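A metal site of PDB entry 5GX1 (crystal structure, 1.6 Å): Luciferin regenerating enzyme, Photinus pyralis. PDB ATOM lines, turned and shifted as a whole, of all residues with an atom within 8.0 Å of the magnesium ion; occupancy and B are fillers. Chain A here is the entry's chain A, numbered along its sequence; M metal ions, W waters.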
ATOM      1  N   VAL A  19     -22.102  -3.570 -18.511  1.00  0.00           N
ATOM      2  CA  VAL A  19     -21.212  -4.666 -18.854  1.00  0.00           C
ATOM      3  C   VAL A  19     -20.500  -4.297 -20.152  1.00  0.00           C
ATOM      4  O   VAL A  19     -20.933  -4.681 -21.243  1.00  0.00           O
ATOM      5  CB  VAL A  19     -21.936  -6.016 -18.998  1.00  0.00           C
ATOM      6  CG1 VAL A  19     -20.921  -7.151 -19.209  1.00  0.00           C
ATOM      7  CG2 VAL A  19     -22.828  -6.330 -17.780  1.00  0.00           C
ATOM      8  N   GLY A  20     -19.443  -3.498 -20.060  1.00  0.00           N
ATOM      9  CA  GLY A  20     -18.616  -3.261 -21.234  1.00  0.00           C
ATOM     10  C   GLY A  20     -17.977  -4.572 -21.678  1.00  0.00           C
ATOM     11  O   GLY A  20     -17.617  -5.412 -20.858  1.00  0.00           O
ATOM     12  N   GLU A  21     -17.863  -4.754 -22.999  1.00  0.00           N
ATOM     13  CA  GLU A  21     -17.545  -6.075 -23.554  1.00  0.00           C
ATOM     14  C   GLU A  21     -17.109  -5.954 -25.010  1.00  0.00           C
ATOM     15  O   GLU A  21     -17.211  -4.901 -25.636  1.00  0.00           O
ATOM     16  CB  GLU A  21     -18.761  -7.010 -23.474  1.00  0.00           C
ATOM     17  CG  GLU A  21     -18.725  -8.007 -22.303  1.00  0.00           C
ATOM     18  CD  GLU A  21     -17.756  -9.143 -22.513  1.00  0.00           C
ATOM     19  OE1 GLU A  21     -17.840 -10.132 -21.749  1.00  0.00           O
ATOM     20  OE2 GLU A  21     -16.913  -9.059 -23.429  1.00  0.00           O
ATOM     21  N   GLY A  22     -16.651  -7.093 -25.553  1.00  0.00           N
ATOM     22  CA  GLY A  22     -16.380  -7.235 -26.975  1.00  0.00           C
ATOM     23  C   GLY A  22     -15.479  -6.197 -27.620  1.00  0.00           C
ATOM     24  O   GLY A  22     -15.771  -5.700 -28.716  1.00  0.00           O
ATOM     25  N   PRO A  23     -14.354  -5.849 -26.994  1.00  0.00           N
ATOM     26  CA  PRO A  23     -13.474  -4.852 -27.609  1.00  0.00           C
ATOM     27  C   PRO A  23     -12.844  -5.354 -28.904  1.00  0.00           C
ATOM     28  O   PRO A  23     -12.423  -6.509 -28.992  1.00  0.00           O
ATOM     29  CB  PRO A  23     -12.397  -4.613 -26.537  1.00  0.00           C
ATOM     30  CG  PRO A  23     -12.342  -5.915 -25.795  1.00  0.00           C
ATOM     31  CD  PRO A  23     -13.757  -6.415 -25.759  1.00  0.00           C
ATOM     32  N   THR A  37     -23.222  -5.430 -23.100  1.00  0.00           N
ATOM     33  CA  THR A  37     -24.074  -6.590 -23.360  1.00  0.00           C
ATOM     34  C   THR A  37     -25.419  -6.511 -22.654  1.00  0.00           C
ATOM     35  O   THR A  37     -26.291  -7.353 -22.930  1.00  0.00           O
ATOM     36  CB  THR A  37     -23.379  -7.896 -22.948  1.00  0.00           C
ATOM     37  OG1 THR A  37     -22.920  -7.804 -21.586  1.00  0.00           O
ATOM     38  CG2 THR A  37     -22.199  -8.187 -23.853  1.00  0.00           C
ATOM     39  N   SER A  62     -23.700  -8.249 -28.370  1.00  0.00           N
ATOM     40  CA  SER A  62     -22.534  -8.848 -27.721  1.00  0.00           C
ATOM     41  C   SER A  62     -21.210  -8.754 -28.487  1.00  0.00           C
ATOM     42  O   SER A  62     -20.176  -9.076 -27.904  1.00  0.00           O
ATOM     43  CB  SER A  62     -22.828 -10.320 -27.386  1.00  0.00           C
ATOM     44  OG  SER A  62     -23.079 -11.073 -28.568  1.00  0.00           O
ATOM     45  N   ASN A 113     -23.456 -14.448 -27.360  1.00  0.00           N
ATOM     46  CA  ASN A 113     -22.507 -13.776 -26.475  1.00  0.00           C
ATOM     47  C   ASN A 113     -21.204 -13.521 -27.221  1.00  0.00           C
ATOM     48  O   ASN A 113     -21.230 -12.918 -28.299  1.00  0.00           O
ATOM     49  CB  ASN A 113     -22.270 -14.556 -25.174  1.00  0.00           C
ATOM     50  CG  ASN A 113     -21.656 -13.686 -24.086  1.00  0.00           C
ATOM     51  OD1 ASN A 113     -21.807 -12.458 -24.111  1.00  0.00           O
ATOM     52  ND2 ASN A 113     -20.969 -14.302 -23.122  1.00  0.00           N
ATOM     53  N   ASP A 114     -20.051 -13.953 -26.703  1.00  0.00           N
ATOM     54  CA  ASP A 114     -18.810 -13.453 -27.285  1.00  0.00           C
ATOM     55  C   ASP A 114     -18.609 -13.994 -28.700  1.00  0.00           C
ATOM     56  O   ASP A 114     -19.069 -15.079 -29.053  1.00  0.00           O
ATOM     57  CB  ASP A 114     -17.618 -13.804 -26.376  1.00  0.00           C
ATOM     58  CG  ASP A 114     -16.465 -12.828 -26.517  1.00  0.00           C
ATOM     59  OD1 ASP A 114     -16.578 -11.853 -27.287  1.00  0.00           O
ATOM     60  OD2 ASP A 114     -15.430 -13.050 -25.830  1.00  0.00           O
ATOM     61  N   GLY A 115     -17.966 -13.181 -29.531  1.00  0.00           N
ATOM     62  CA  GLY A 115     -17.706 -13.555 -30.912  1.00  0.00           C
ATOM     63  C   GLY A 115     -16.463 -12.849 -31.413  1.00  0.00           C
ATOM     64  O   GLY A 115     -16.085 -11.783 -30.910  1.00  0.00           O
ATOM     65  N   MET A 128     -25.911 -18.516 -25.135  1.00  0.00           N
ATOM     66  CA  MET A 128     -26.131 -18.749 -23.718  1.00  0.00           C
ATOM     67  C   MET A 128     -27.589 -18.438 -23.409  1.00  0.00           C
ATOM     68  O   MET A 128     -28.237 -17.672 -24.118  1.00  0.00           O
ATOM     69  CB  MET A 128     -25.229 -17.854 -22.858  1.00  0.00           C
ATOM     70  CG  MET A 128     -25.539 -16.370 -23.072  1.00  0.00           C
ATOM     71  SD  MET A 128     -24.461 -15.183 -22.219  1.00  0.00           S
ATOM     72  CE  MET A 128     -25.160 -15.217 -20.564  1.00  0.00           C
ATOM     73  N   ILE A 161     -21.919 -20.256 -20.577  1.00  0.00           N
ATOM     74  CA  ILE A 161     -21.730 -18.856 -20.944  1.00  0.00           C
ATOM     75  C   ILE A 161     -20.626 -18.794 -21.995  1.00  0.00           C
ATOM     76  O   ILE A 161     -19.435 -18.849 -21.670  1.00  0.00           O
ATOM     77  CB  ILE A 161     -21.406 -17.964 -19.732  1.00  0.00           C
ATOM     78  CG1 ILE A 161     -22.544 -18.020 -18.707  1.00  0.00           C
ATOM     79  CG2 ILE A 161     -21.226 -16.508 -20.192  1.00  0.00           C
ATOM     80  CD1 ILE A 161     -22.342 -17.128 -17.486  1.00  0.00           C
ATOM     81  N   ALA A 162     -21.028 -18.698 -23.268  1.00  0.00           N
ATOM     82  CA  ALA A 162     -20.106 -18.706 -24.403  1.00  0.00           C
ATOM     83  C   ALA A 162     -19.204 -17.477 -24.379  1.00  0.00           C
ATOM     84  O   ALA A 162     -19.699 -16.351 -24.461  1.00  0.00           O
ATOM     85  CB  ALA A 162     -20.916 -18.747 -25.693  1.00  0.00           C
ATOM     86  N   ASN A 163     -17.899 -17.685 -24.264  1.00  0.00           N
ATOM     87  CA  ASN A 163     -17.048 -16.511 -24.069  1.00  0.00           C
ATOM     88  C   ASN A 163     -15.778 -16.523 -24.931  1.00  0.00           C
ATOM     89  O   ASN A 163     -15.867 -16.810 -26.129  1.00  0.00           O
ATOM     90  CB  ASN A 163     -16.757 -16.341 -22.575  1.00  0.00           C
ATOM     91  CG  ASN A 163     -17.503 -15.157 -22.011  1.00  0.00           C
ATOM     92  OD1 ASN A 163     -17.597 -14.132 -22.675  1.00  0.00           O
ATOM     93  ND2 ASN A 163     -18.053 -15.291 -20.808  1.00  0.00           N
ATOM     94  N   GLY A 164     -14.619 -16.158 -24.382  1.00  0.00           N
ATOM     95  CA  GLY A 164     -13.509 -15.674 -25.220  1.00  0.00           C
ATOM     96  C   GLY A 164     -12.958 -16.713 -26.190  1.00  0.00           C
ATOM     97  O   GLY A 164     -12.916 -17.912 -25.922  1.00  0.00           O
ATOM     98  N   ILE A 177     -13.419 -20.442 -24.217  1.00  0.00           N
ATOM     99  CA  ILE A 177     -13.828 -20.294 -22.825  1.00  0.00           C
ATOM    100  C   ILE A 177     -15.343 -20.421 -22.712  1.00  0.00           C
ATOM    101  O   ILE A 177     -16.090 -19.645 -23.325  1.00  0.00           O
ATOM    102  CB  ILE A 177     -13.375 -18.943 -22.246  1.00  0.00           C
ATOM    103  CG1 ILE A 177     -11.859 -18.901 -22.087  1.00  0.00           C
ATOM    104  CG2 ILE A 177     -14.081 -18.675 -20.896  1.00  0.00           C
ATOM    105  CD1 ILE A 177     -11.314 -17.478 -21.998  1.00  0.00           C
ATOM    106  N   SER A 179     -17.420 -19.765 -19.445  1.00  0.00           N
ATOM    107  CA  SER A 179     -17.108 -19.265 -18.099  1.00  0.00           C
ATOM    108  C   SER A 179     -17.482 -20.268 -17.030  1.00  0.00           C
ATOM    109  O   SER A 179     -16.800 -20.361 -15.992  1.00  0.00           O
ATOM    110  CB  SER A 179     -17.828 -17.941 -17.851  1.00  0.00           C
ATOM    111  OG  SER A 179     -17.334 -16.930 -18.723  1.00  0.00           O
ATOM    112  N   PRO A 214     -13.094 -17.128 -16.102  1.00  0.00           N
ATOM    113  CA  PRO A 214     -12.556 -16.639 -17.379  1.00  0.00           C
ATOM    114  C   PRO A 214     -13.692 -16.078 -18.229  1.00  0.00           C
ATOM    115  O   PRO A 214     -14.804 -16.609 -18.223  1.00  0.00           O
ATOM    116  CB  PRO A 214     -11.932 -17.888 -18.001  1.00  0.00           C
ATOM    117  CG  PRO A 214     -12.766 -19.019 -17.455  1.00  0.00           C
ATOM    118  CD  PRO A 214     -13.117 -18.597 -16.038  1.00  0.00           C
ATOM    119  N   ASP A 215     -13.407 -14.977 -18.924  1.00  0.00           N
ATOM    120  CA  ASP A 215     -14.439 -14.280 -19.689  1.00  0.00           C
ATOM    121  C   ASP A 215     -13.906 -14.121 -21.110  1.00  0.00           C
ATOM    122  O   ASP A 215     -13.759 -15.120 -21.812  1.00  0.00           O
ATOM    123  CB  ASP A 215     -14.795 -12.953 -18.988  1.00  0.00           C
ATOM    124  CG  ASP A 215     -16.154 -12.390 -19.405  1.00  0.00           C
ATOM    125  OD1 ASP A 215     -16.583 -12.618 -20.545  1.00  0.00           O
ATOM    126  OD2 ASP A 215     -16.797 -11.699 -18.564  1.00  0.00           O
ATOM    127  N   GLY A 216     -13.577 -12.895 -21.561  1.00  0.00           N
ATOM    128  CA  GLY A 216     -12.945 -12.734 -22.864  1.00  0.00           C
ATOM    129  C   GLY A 216     -11.458 -13.120 -22.842  1.00  0.00           C
ATOM    130  O   GLY A 216     -10.841 -13.215 -21.789  1.00  0.00           O
ATOM    131  N   GLN A 217     -10.873 -13.343 -24.023  1.00  0.00           N
ATOM    132  CA  GLN A 217      -9.433 -13.558 -24.085  1.00  0.00           C
ATOM    133  C   GLN A 217      -8.874 -13.102 -25.422  1.00  0.00           C
ATOM    134  O   GLN A 217      -9.608 -12.910 -26.403  1.00  0.00           O
ATOM    135  CB  GLN A 217      -9.051 -15.028 -23.857  1.00  0.00           C
ATOM    136  CG  GLN A 217      -9.513 -15.983 -24.964  1.00  0.00           C
ATOM    137  CD  GLN A 217      -9.116 -17.418 -24.687  1.00  0.00           C
ATOM    138  OE1 GLN A 217      -8.129 -17.681 -23.994  1.00  0.00           O
ATOM    139  NE2 GLN A 217      -9.899 -18.362 -25.209  1.00  0.00           N
ATOM    140  N   ALA A 228      -9.310 -12.347 -19.431  1.00  0.00           N
ATOM    141  CA  ALA A 228     -10.056 -11.514 -18.493  1.00  0.00           C
ATOM    142  C   ALA A 228     -10.644 -12.375 -17.380  1.00  0.00           C
ATOM    143  O   ALA A 228     -11.223 -13.427 -17.642  1.00  0.00           O
ATOM    144  CB  ALA A 228     -11.177 -10.782 -19.227  1.00  0.00           C
ATOM    145  N   PHE A 230     -13.356 -12.329 -14.641  1.00  0.00           N
ATOM    146  CA  PHE A 230     -14.560 -11.704 -14.083  1.00  0.00           C
ATOM    147  C   PHE A 230     -14.692 -12.122 -12.625  1.00  0.00           C
ATOM    148  O   PHE A 230     -14.701 -13.317 -12.313  1.00  0.00           O
ATOM    149  CB  PHE A 230     -15.785 -12.125 -14.913  1.00  0.00           C
ATOM    150  CG  PHE A 230     -17.045 -11.388 -14.571  1.00  0.00           C
ATOM    151  CD1 PHE A 230     -17.439 -10.280 -15.318  1.00  0.00           C
ATOM    152  CD2 PHE A 230     -17.851 -11.804 -13.514  1.00  0.00           C
ATOM    153  CE1 PHE A 230     -18.608  -9.602 -15.003  1.00  0.00           C
ATOM    154  CE2 PHE A 230     -19.016 -11.109 -13.200  1.00  0.00           C
ATOM    155  CZ  PHE A 230     -19.397 -10.016 -13.945  1.00  0.00           C
ATOM    156  N   VAL A 257     -13.626  -7.767 -14.496  1.00  0.00           N
ATOM    157  CA  VAL A 257     -12.932  -7.653 -15.773  1.00  0.00           C
ATOM    158  C   VAL A 257     -13.612  -8.569 -16.786  1.00  0.00           C
ATOM    159  O   VAL A 257     -13.862  -9.740 -16.495  1.00  0.00           O
ATOM    160  CB  VAL A 257     -11.449  -8.030 -15.602  1.00  0.00           C
ATOM    161  CG1 VAL A 257     -10.708  -7.882 -16.921  1.00  0.00           C
ATOM    162  CG2 VAL A 257     -10.799  -7.168 -14.517  1.00  0.00           C
ATOM    163  N   THR A 258     -13.935  -8.035 -17.975  1.00  0.00           N
ATOM    164  CA  THR A 258     -14.755  -8.754 -18.934  1.00  0.00           C
ATOM    165  C   THR A 258     -14.014  -9.191 -20.194  1.00  0.00           C
ATOM    166  O   THR A 258     -14.214 -10.319 -20.651  1.00  0.00           O
ATOM    167  CB  THR A 258     -15.983  -7.924 -19.354  1.00  0.00           C
ATOM    168  OG1 THR A 258     -15.557  -6.676 -19.925  1.00  0.00           O
ATOM    169  CG2 THR A 258     -16.885  -7.667 -18.138  1.00  0.00           C
ATOM    170  N   SER A 259     -13.175  -8.349 -20.792  1.00  0.00           N
ATOM    171  CA  SER A 259     -12.510  -8.778 -22.011  1.00  0.00           C
ATOM    172  C   SER A 259     -11.291  -7.903 -22.286  1.00  0.00           C
ATOM    173  O   SER A 259     -10.979  -6.983 -21.520  1.00  0.00           O
ATOM    174  CB  SER A 259     -13.464  -8.768 -23.207  1.00  0.00           C
ATOM    175  OG  SER A 259     -12.913  -9.539 -24.264  1.00  0.00           O
ATOM    176  N   THR A 273     -11.927  -4.115 -20.898  1.00  0.00           N
ATOM    177  CA  THR A 273     -13.278  -3.723 -20.521  1.00  0.00           C
ATOM    178  C   THR A 273     -13.661  -4.343 -19.172  1.00  0.00           C
ATOM    179  O   THR A 273     -13.050  -5.324 -18.712  1.00  0.00           O
ATOM    180  CB  THR A 273     -14.286  -4.144 -21.598  1.00  0.00           C
ATOM    181  OG1 THR A 273     -14.117  -5.529 -21.928  1.00  0.00           O
ATOM    182  CG2 THR A 273     -14.111  -3.304 -22.881  1.00  0.00           C
HETATM  183 MG    MG M   1     -17.688 -12.098 -22.208  1.00  0.00          MG
HETATM  184  O   HOH W   1     -19.008 -11.708 -23.905  1.00  0.00           O
HETATM  185  O   HOH W   2     -19.597 -12.374 -21.218  1.00  0.00           O
HETATM  186  O   HOH W   3     -16.067 -11.654 -23.395  1.00  0.00           O
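The side-chain amide oxygen of Asn 163 sits close to the side-chain amide nitrogen of Asn 113 (3.4 Å).
N of Asp 215 lies within hydrogen-bond range of O of Ala 228 (3.0 Å).
O of Asp 215 lies within hydrogen-bond range of N of Gly 164, 2.9 Å away.
ND2 of Asn 163 is in hydrogen-bond range of OG of Ser 179 (2.7 Å).
O of Ile 177 lies within hydrogen-bond range of N of Asn 163.
The nearest printed residue that does not touch the magnesium ion is Asn 113 (4.1 Å).
The magnesium ion is bound by OE1 of Glu 21 (2.0 Å), water W3 (2.1 Å), OD1 of Asp 215 (2.1 Å), OD1 of Asn 163 (2.1 Å), water W2 (2.2 Å) and water W1 (2.2 Å).
The magnesium ion has six donor atoms within binding distance.
Water W1 bridges OD1 of Asn 113 (2.9 Å) and OE2 of Glu 21 (3.4 Å).
Water W2 bridges ND2 of Asn 113 (3.0 Å) and ND2 of Asn 163 (3.3 Å).
Water W3 lies within hydrogen-bond range of the side-chain carboxylate of Glu 21, the side-chain carboxylate of Asp 114 and the backbone NH of Gly 216.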
